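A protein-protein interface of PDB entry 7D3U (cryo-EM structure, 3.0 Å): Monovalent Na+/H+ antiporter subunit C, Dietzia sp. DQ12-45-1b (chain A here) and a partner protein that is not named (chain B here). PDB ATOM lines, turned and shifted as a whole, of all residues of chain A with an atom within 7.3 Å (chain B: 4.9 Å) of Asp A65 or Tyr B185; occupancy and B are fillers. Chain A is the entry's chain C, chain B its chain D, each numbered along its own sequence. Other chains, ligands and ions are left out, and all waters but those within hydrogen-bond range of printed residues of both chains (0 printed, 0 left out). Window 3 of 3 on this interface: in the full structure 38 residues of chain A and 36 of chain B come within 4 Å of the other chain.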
ATOM      1  N   LEU A  41     -16.069 -31.525  11.093  1.00  0.00           N
ATOM      2  CA  LEU A  41     -15.970 -30.111  10.746  1.00  0.00           C
ATOM      3  C   LEU A  41     -14.772 -29.468  11.428  1.00  0.00           C
ATOM      4  O   LEU A  41     -14.044 -28.686  10.809  1.00  0.00           O
ATOM      5  CB  LEU A  41     -17.254 -29.380  11.128  1.00  0.00           C
ATOM      6  CG  LEU A  41     -18.198 -28.991   9.993  1.00  0.00           C
ATOM      7  CD1 LEU A  41     -19.453 -28.364  10.560  1.00  0.00           C
ATOM      8  CD2 LEU A  41     -17.512 -28.035   9.041  1.00  0.00           C
ATOM      9  N   MET A  42     -14.553 -29.786  12.706  1.00  0.00           N
ATOM     10  CA  MET A  42     -13.376 -29.271  13.399  1.00  0.00           C
ATOM     11  C   MET A  42     -12.090 -29.850  12.825  1.00  0.00           C
ATOM     12  O   MET A  42     -11.034 -29.215  12.914  1.00  0.00           O
ATOM     13  CB  MET A  42     -13.466 -29.566  14.894  1.00  0.00           C
ATOM     14  CG  MET A  42     -14.304 -28.570  15.670  1.00  0.00           C
ATOM     15  SD  MET A  42     -13.830 -26.862  15.367  1.00  0.00           S
ATOM     16  CE  MET A  42     -12.115 -26.890  15.872  1.00  0.00           C
ATOM     17  N   ALA A  43     -12.156 -31.046  12.237  1.00  0.00           N
ATOM     18  CA  ALA A  43     -10.980 -31.633  11.609  1.00  0.00           C
ATOM     19  C   ALA A  43     -10.642 -30.972  10.283  1.00  0.00           C
ATOM     20  O   ALA A  43      -9.475 -30.987   9.879  1.00  0.00           O
ATOM     21  CB  ALA A  43     -11.187 -33.131  11.394  1.00  0.00           C
ATOM     22  N   ALA A  44     -11.628 -30.386   9.603  1.00  0.00           N
ATOM     23  CA  ALA A  44     -11.371 -29.782   8.301  1.00  0.00           C
ATOM     24  C   ALA A  44     -10.524 -28.526   8.421  1.00  0.00           C
ATOM     25  O   ALA A  44      -9.843 -28.147   7.462  1.00  0.00           O
ATOM     26  CB  ALA A  44     -12.689 -29.465   7.600  1.00  0.00           C
ATOM     27  N   GLY A  45     -10.544 -27.873   9.578  1.00  0.00           N
ATOM     28  CA  GLY A  45      -9.756 -26.674   9.778  1.00  0.00           C
ATOM     29  C   GLY A  45      -8.299 -26.960  10.067  1.00  0.00           C
ATOM     30  O   GLY A  45      -7.640 -26.201  10.783  1.00  0.00           O
ATOM     31  N   GLY A  46      -7.782 -28.054   9.516  1.00  0.00           N
ATOM     32  CA  GLY A  46      -6.400 -28.422   9.729  1.00  0.00           C
ATOM     33  C   GLY A  46      -6.203 -29.352  10.906  1.00  0.00           C
ATOM     34  O   GLY A  46      -5.641 -30.440  10.754  1.00  0.00           O
ATOM     35  N   ALA A  47      -6.639 -28.914  12.089  1.00  0.00           N
ATOM     36  CA  ALA A  47      -6.522 -29.673  13.331  1.00  0.00           C
ATOM     37  C   ALA A  47      -5.067 -29.895  13.725  1.00  0.00           C
ATOM     38  O   ALA A  47      -4.786 -30.586  14.709  1.00  0.00           O
ATOM     39  CB  ALA A  47      -7.253 -31.013  13.224  1.00  0.00           C
ATOM     40  N   ARG A  49      -3.256 -27.056  14.115  1.00  0.00           N
ATOM     41  CA  ARG A  49      -3.047 -25.802  14.830  1.00  0.00           C
ATOM     42  C   ARG A  49      -4.021 -25.786  15.999  1.00  0.00           C
ATOM     43  O   ARG A  49      -5.234 -25.666  15.799  1.00  0.00           O
ATOM     44  CB  ARG A  49      -3.263 -24.605  13.906  1.00  0.00           C
ATOM     45  CG  ARG A  49      -2.414 -24.637  12.649  1.00  0.00           C
ATOM     46  CD  ARG A  49      -2.914 -23.640  11.622  1.00  0.00           C
ATOM     47  NE  ARG A  49      -4.188 -24.050  11.044  1.00  0.00           N
ATOM     48  CZ  ARG A  49      -4.306 -24.905  10.034  1.00  0.00           C
ATOM     49  NH1 ARG A  49      -3.225 -25.440   9.487  1.00  0.00           N
ATOM     50  NH2 ARG A  49      -5.505 -25.223   9.571  1.00  0.00           N
ATOM     51  N   GLU A  51      -4.091 -23.704  18.728  1.00  0.00           N
ATOM     52  CA  GLU A  51      -4.181 -22.457  19.471  1.00  0.00           C
ATOM     53  C   GLU A  51      -5.497 -21.761  19.156  1.00  0.00           C
ATOM     54  O   GLU A  51      -5.943 -21.745  18.006  1.00  0.00           O
ATOM     55  CB  GLU A  51      -3.006 -21.537  19.144  1.00  0.00           C
ATOM     56  CG  GLU A  51      -2.693 -20.532  20.237  1.00  0.00           C
ATOM     57  CD  GLU A  51      -1.351 -19.859  20.046  1.00  0.00           C
ATOM     58  OE1 GLU A  51      -0.733 -20.056  18.979  1.00  0.00           O
ATOM     59  OE2 GLU A  51      -0.912 -19.133  20.961  1.00  0.00           O
ATOM     60  N   PRO A  53      -8.164 -18.878  18.364  1.00  0.00           N
ATOM     61  CA  PRO A  53      -8.099 -17.598  17.651  1.00  0.00           C
ATOM     62  C   PRO A  53      -8.727 -16.448  18.431  1.00  0.00           C
ATOM     63  O   PRO A  53      -9.560 -15.698  17.915  1.00  0.00           O
ATOM     64  CB  PRO A  53      -8.876 -17.896  16.361  1.00  0.00           C
ATOM     65  CG  PRO A  53      -9.901 -18.876  16.795  1.00  0.00           C
ATOM     66  CD  PRO A  53      -9.256 -19.729  17.863  1.00  0.00           C
ATOM     67  N   LEU A  62      -0.429 -21.131  13.213  1.00  0.00           N
ATOM     68  CA  LEU A  62      -0.322 -21.604  14.585  1.00  0.00           C
ATOM     69  C   LEU A  62      -1.650 -21.665  15.323  1.00  0.00           C
ATOM     70  O   LEU A  62      -1.756 -22.433  16.286  1.00  0.00           O
ATOM     71  CB  LEU A  62       0.645 -20.718  15.385  1.00  0.00           C
ATOM     72  CG  LEU A  62       1.248 -21.330  16.649  1.00  0.00           C
ATOM     73  CD1 LEU A  62       1.950 -22.636  16.325  1.00  0.00           C
ATOM     74  CD2 LEU A  62       2.203 -20.353  17.314  1.00  0.00           C
ATOM     75  N   THR A  63      -2.660 -20.903  14.910  1.00  0.00           N
ATOM     76  CA  THR A  63      -3.959 -20.896  15.564  1.00  0.00           C
ATOM     77  C   THR A  63      -4.981 -21.672  14.744  1.00  0.00           C
ATOM     78  O   THR A  63      -4.892 -21.752  13.517  1.00  0.00           O
ATOM     79  CB  THR A  63      -4.465 -19.470  15.781  1.00  0.00           C
ATOM     80  OG1 THR A  63      -5.058 -18.986  14.570  1.00  0.00           O
ATOM     81  CG2 THR A  63      -3.330 -18.556  16.193  1.00  0.00           C
ATOM     82  N   SER A  64      -5.959 -22.241  15.443  1.00  0.00           N
ATOM     83  CA  SER A  64      -7.012 -22.998  14.783  1.00  0.00           C
ATOM     84  C   SER A  64      -7.854 -22.082  13.907  1.00  0.00           C
ATOM     85  O   SER A  64      -8.071 -20.908  14.221  1.00  0.00           O
ATOM     86  CB  SER A  64      -7.897 -23.693  15.816  1.00  0.00           C
ATOM     87  OG  SER A  64      -9.115 -24.125  15.236  1.00  0.00           O
ATOM     88  N   ASP A  65      -8.330 -22.628  12.794  1.00  0.00           N
ATOM     89  CA  ASP A  65      -9.116 -21.840  11.859  1.00  0.00           C
ATOM     90  C   ASP A  65     -10.490 -21.533  12.445  1.00  0.00           C
ATOM     91  O   ASP A  65     -11.080 -22.342  13.165  1.00  0.00           O
ATOM     92  CB  ASP A  65      -9.242 -22.579  10.528  1.00  0.00           C
ATOM     93  CG  ASP A  65      -9.944 -21.761   9.475  1.00  0.00           C
ATOM     94  OD1 ASP A  65      -9.992 -20.524   9.625  1.00  0.00           O
ATOM     95  OD2 ASP A  65     -10.466 -22.353   8.509  1.00  0.00           O
ATOM     96  N   GLY A  66     -10.998 -20.344  12.130  1.00  0.00           N
ATOM     97  CA  GLY A  66     -12.225 -19.858  12.732  1.00  0.00           C
ATOM     98  C   GLY A  66     -13.493 -20.200  11.976  1.00  0.00           C
ATOM     99  O   GLY A  66     -14.570 -20.298  12.573  1.00  0.00           O
ATOM    100  N   LEU A  67     -13.382 -20.381  10.657  1.00  0.00           N
ATOM    101  CA  LEU A  67     -14.575 -20.678   9.864  1.00  0.00           C
ATOM    102  C   LEU A  67     -15.178 -22.033  10.208  1.00  0.00           C
ATOM    103  O   LEU A  67     -16.406 -22.106  10.394  1.00  0.00           O
ATOM    104  CB  LEU A  67     -14.257 -20.558   8.371  1.00  0.00           C
ATOM    105  CG  LEU A  67     -15.498 -20.582   7.480  1.00  0.00           C
ATOM    106  CD1 LEU A  67     -16.438 -19.465   7.875  1.00  0.00           C
ATOM    107  CD2 LEU A  67     -15.125 -20.472   6.016  1.00  0.00           C
ATOM    108  N   PRO A  68     -14.418 -23.131  10.298  1.00  0.00           N
ATOM    109  CA  PRO A  68     -15.041 -24.386  10.742  1.00  0.00           C
ATOM    110  C   PRO A  68     -15.549 -24.317  12.166  1.00  0.00           C
ATOM    111  O   PRO A  68     -16.513 -25.016  12.503  1.00  0.00           O
ATOM    112  CB  PRO A  68     -13.911 -25.411  10.590  1.00  0.00           C
ATOM    113  CG  PRO A  68     -12.677 -24.614  10.688  1.00  0.00           C
ATOM    114  CD  PRO A  68     -12.993 -23.332   9.988  1.00  0.00           C
ATOM    115  N   GLN A  69     -14.945 -23.480  13.011  1.00  0.00           N
ATOM    116  CA  GLN A  69     -15.462 -23.313  14.364  1.00  0.00           C
ATOM    117  C   GLN A  69     -16.828 -22.642  14.348  1.00  0.00           C
ATOM    118  O   GLN A  69     -17.734 -23.055  15.077  1.00  0.00           O
ATOM    119  CB  GLN A  69     -14.472 -22.518  15.212  1.00  0.00           C
ATOM    120  CG  GLN A  69     -13.183 -23.267  15.489  1.00  0.00           C
ATOM    121  CD  GLN A  69     -12.346 -22.615  16.566  1.00  0.00           C
ATOM    122  OE1 GLN A  69     -11.131 -22.798  16.618  1.00  0.00           O
ATOM    123  NE2 GLN A  69     -12.994 -21.860  17.440  1.00  0.00           N
ATOM    124  N   ALA A  70     -17.006 -21.621  13.510  1.00  0.00           N
ATOM    125  CA  ALA A  70     -18.336 -21.041  13.347  1.00  0.00           C
ATOM    126  C   ALA A  70     -19.305 -22.054  12.750  1.00  0.00           C
ATOM    127  O   ALA A  70     -20.486 -22.094  13.122  1.00  0.00           O
ATOM    128  CB  ALA A  70     -18.262 -19.791  12.475  1.00  0.00           C
ATOM    129  N   PHE A  71     -18.821 -22.884  11.826  1.00  0.00           N
ATOM    130  CA  PHE A  71     -19.671 -23.900  11.216  1.00  0.00           C
ATOM    131  C   PHE A  71     -20.216 -24.862  12.263  1.00  0.00           C
ATOM    132  O   PHE A  71     -21.422 -25.130  12.311  1.00  0.00           O
ATOM    133  CB  PHE A  71     -18.894 -24.663  10.144  1.00  0.00           C
ATOM    134  CG  PHE A  71     -18.719 -23.905   8.861  1.00  0.00           C
ATOM    135  CD1 PHE A  71     -19.161 -22.601   8.741  1.00  0.00           C
ATOM    136  CD2 PHE A  71     -18.111 -24.502   7.773  1.00  0.00           C
ATOM    137  CE1 PHE A  71     -18.997 -21.909   7.561  1.00  0.00           C
ATOM    138  CE2 PHE A  71     -17.945 -23.813   6.592  1.00  0.00           C
ATOM    139  CZ  PHE A  71     -18.389 -22.515   6.486  1.00  0.00           C
ATOM    140  N   VAL B 181     -19.877 -31.087   3.190  1.00  0.00           N
ATOM    141  CA  VAL B 181     -19.364 -29.720   3.186  1.00  0.00           C
ATOM    142  C   VAL B 181     -18.073 -29.637   3.990  1.00  0.00           C
ATOM    143  O   VAL B 181     -17.124 -28.942   3.606  1.00  0.00           O
ATOM    144  CB  VAL B 181     -20.433 -28.751   3.722  1.00  0.00           C
ATOM    145  CG1 VAL B 181     -19.810 -27.428   4.126  1.00  0.00           C
ATOM    146  CG2 VAL B 181     -21.516 -28.535   2.684  1.00  0.00           C
ATOM    147  N   ALA B 182     -18.009 -30.360   5.110  1.00  0.00           N
ATOM    148  CA  ALA B 182     -16.795 -30.372   5.915  1.00  0.00           C
ATOM    149  C   ALA B 182     -15.629 -30.972   5.145  1.00  0.00           C
ATOM    150  O   ALA B 182     -14.512 -30.451   5.192  1.00  0.00           O
ATOM    151  CB  ALA B 182     -17.033 -31.146   7.210  1.00  0.00           C
ATOM    152  N   LEU B 183     -15.870 -32.057   4.412  1.00  0.00           N
ATOM    153  CA  LEU B 183     -14.787 -32.669   3.650  1.00  0.00           C
ATOM    154  C   LEU B 183     -14.369 -31.801   2.470  1.00  0.00           C
ATOM    155  O   LEU B 183     -13.181 -31.755   2.128  1.00  0.00           O
ATOM    156  CB  LEU B 183     -15.196 -34.062   3.177  1.00  0.00           C
ATOM    157  CG  LEU B 183     -15.437 -35.088   4.285  1.00  0.00           C
ATOM    158  CD1 LEU B 183     -15.740 -36.450   3.697  1.00  0.00           C
ATOM    159  CD2 LEU B 183     -14.239 -35.160   5.212  1.00  0.00           C
ATOM    160  N   ILE B 184     -15.319 -31.103   1.843  1.00  0.00           N
ATOM    161  CA  ILE B 184     -14.965 -30.157   0.787  1.00  0.00           C
ATOM    162  C   ILE B 184     -14.094 -29.043   1.347  1.00  0.00           C
ATOM    163  O   ILE B 184     -13.087 -28.658   0.742  1.00  0.00           O
ATOM    164  CB  ILE B 184     -16.231 -29.596   0.114  1.00  0.00           C
ATOM    165  CG1 ILE B 184     -16.953 -30.688  -0.667  1.00  0.00           C
ATOM    166  CG2 ILE B 184     -15.876 -28.454  -0.813  1.00  0.00           C
ATOM    167  CD1 ILE B 184     -18.151 -30.190  -1.431  1.00  0.00           C
ATOM    168  N   TYR B 185     -14.463 -28.510   2.513  1.00  0.00           N
ATOM    169  CA  TYR B 185     -13.647 -27.475   3.138  1.00  0.00           C
ATOM    170  C   TYR B 185     -12.303 -28.024   3.597  1.00  0.00           C
ATOM    171  O   TYR B 185     -11.333 -27.269   3.712  1.00  0.00           O
ATOM    172  CB  TYR B 185     -14.394 -26.851   4.314  1.00  0.00           C
ATOM    173  CG  TYR B 185     -13.684 -25.669   4.928  1.00  0.00           C
ATOM    174  CD1 TYR B 185     -13.867 -24.391   4.427  1.00  0.00           C
ATOM    175  CD2 TYR B 185     -12.833 -25.830   6.011  1.00  0.00           C
ATOM    176  CE1 TYR B 185     -13.222 -23.309   4.982  1.00  0.00           C
ATOM    177  CE2 TYR B 185     -12.183 -24.754   6.571  1.00  0.00           C
ATOM    178  CZ  TYR B 185     -12.381 -23.497   6.053  1.00  0.00           C
ATOM    179  OH  TYR B 185     -11.736 -22.418   6.611  1.00  0.00           O
ATOM    180  N   GLY B 186     -12.230 -29.321   3.871  1.00  0.00           N
ATOM    181  CA  GLY B 186     -10.984 -29.932   4.280  1.00  0.00           C
ATOM    182  C   GLY B 186     -10.003 -30.104   3.141  1.00  0.00           C
ATOM    183  O   GLY B 186      -8.823 -29.773   3.280  1.00  0.00           O
ATOM    184  N   VAL B 187     -10.478 -30.619   2.007  1.00  0.00           N
ATOM    185  CA  VAL B 187      -9.586 -30.861   0.877  1.00  0.00           C
ATOM    186  C   VAL B 187      -9.312 -29.573   0.108  1.00  0.00           C
ATOM    187  O   VAL B 187      -8.161 -29.267  -0.219  1.00  0.00           O
ATOM    188  CB  VAL B 187     -10.152 -31.974  -0.027  1.00  0.00           C
ATOM    189  CG1 VAL B 187     -10.308 -33.242   0.760  1.00  0.00           C
ATOM    190  CG2 VAL B 187     -11.504 -31.585  -0.565  1.00  0.00           C
ATOM    191  N   THR B 188     -10.352 -28.804  -0.196  1.00  0.00           N
ATOM    192  CA  THR B 188     -10.181 -27.496  -0.804  1.00  0.00           C
ATOM    193  C   THR B 188     -10.037 -26.456   0.302  1.00  0.00           C
ATOM    194  O   THR B 188      -9.835 -26.785   1.472  1.00  0.00           O
ATOM    195  CB  THR B 188     -11.340 -27.171  -1.741  1.00  0.00           C
ATOM    196  OG1 THR B 188     -12.573 -27.225  -1.017  1.00  0.00           O
ATOM    197  CG2 THR B 188     -11.385 -28.154  -2.887  1.00  0.00           C
ATOM    198  N   GLY B 189     -10.130 -25.184  -0.057  1.00  0.00           N
ATOM    199  CA  GLY B 189      -9.972 -24.136   0.926  1.00  0.00           C
ATOM    200  C   GLY B 189     -11.277 -23.507   1.358  1.00  0.00           C
ATOM    201  O   GLY B 189     -11.414 -23.092   2.509  1.00  0.00           O
ATOM    202  N   THR B 190     -12.250 -23.435   0.455  1.00  0.00           N
ATOM    203  CA  THR B 190     -13.465 -22.679   0.704  1.00  0.00           C
ATOM    204  C   THR B 190     -14.693 -23.541   0.460  1.00  0.00           C
ATOM    205  O   THR B 190     -14.650 -24.538  -0.262  1.00  0.00           O
ATOM    206  CB  THR B 190     -13.539 -21.435  -0.182  1.00  0.00           C
ATOM    207  OG1 THR B 190     -13.378 -21.821  -1.551  1.00  0.00           O
ATOM    208  CG2 THR B 190     -12.443 -20.456   0.193  1.00  0.00           C
ATOM    209  N   VAL B 191     -15.799 -23.130   1.082  1.00  0.00           N
ATOM    210  CA  VAL B 191     -17.102 -23.731   0.819  1.00  0.00           C
ATOM    211  C   VAL B 191     -17.898 -22.945  -0.209  1.00  0.00           C
ATOM    212  O   VAL B 191     -18.980 -23.400  -0.615  1.00  0.00           O
ATOM    213  CB  VAL B 191     -17.925 -23.869   2.116  1.00  0.00           C
ATOM    214  CG1 VAL B 191     -17.344 -24.956   2.995  1.00  0.00           C
ATOM    215  CG2 VAL B 191     -17.963 -22.546   2.854  1.00  0.00           C
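The side-chain carboxylate of Asp A65 sits close to the side-chain hydroxyl of Tyr B185, at 2.3 Å.
O of Asp A65 sits close to OE1 of Gln A69 (3.5 Å).
Ala B182 touches Leu A41 (CB to CD2, 3.6 Å). Ala B182 touches Ala A44. Tyr B185 touches Ala A44. Ala A44 touches Gly B186 (CB to N, 3.8 Å). Leu A67 touches Tyr B185. Pro A68 touches Tyr B185. Phe A71 touches Val B191.
Tyr B185 touches just these residues of chain A: Ala A44 (3.97 Å), Asp A65 (2.3 Å), Leu A67 (3.6 Å) and Pro A68 (3.7 Å). Of the printed residues of chain B, Ala A44 touches Ala B182, Tyr B185 and Gly B186. Of the printed residues of chain A, Ala B182 touches Leu A41 (3.6 Å) and Ala A44 (3.2 Å). Of the printed residues of chain B, Phe A71 touches Val B191. Gly A45 touches none of the printed residues of chain B. Ala A47 touches none of the printed residues of chain B. The nearest residue of chain A that does not touch Tyr B185 is Gly A45 (4.5 Å).
Of the 11 printed residues of chain B, 4 touch a printed residue of chain A. Printed residues of chain B that touch a printed residue of chain A: Ala B182, Tyr B185, Gly B186 and Val B191. Printed residues of chain A that touch a printed residue of chain B: Leu A41, Ala A44, Asp A65, Leu A67, Pro A68 and Phe A71. Hydrophobic or aromatic side chains of chain A that line the printed part of chain B: Leu A41, Ala A44, Leu A67, Pro A68 and Phe A71. Among the printed residues, 8 pairs touch across the chains.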
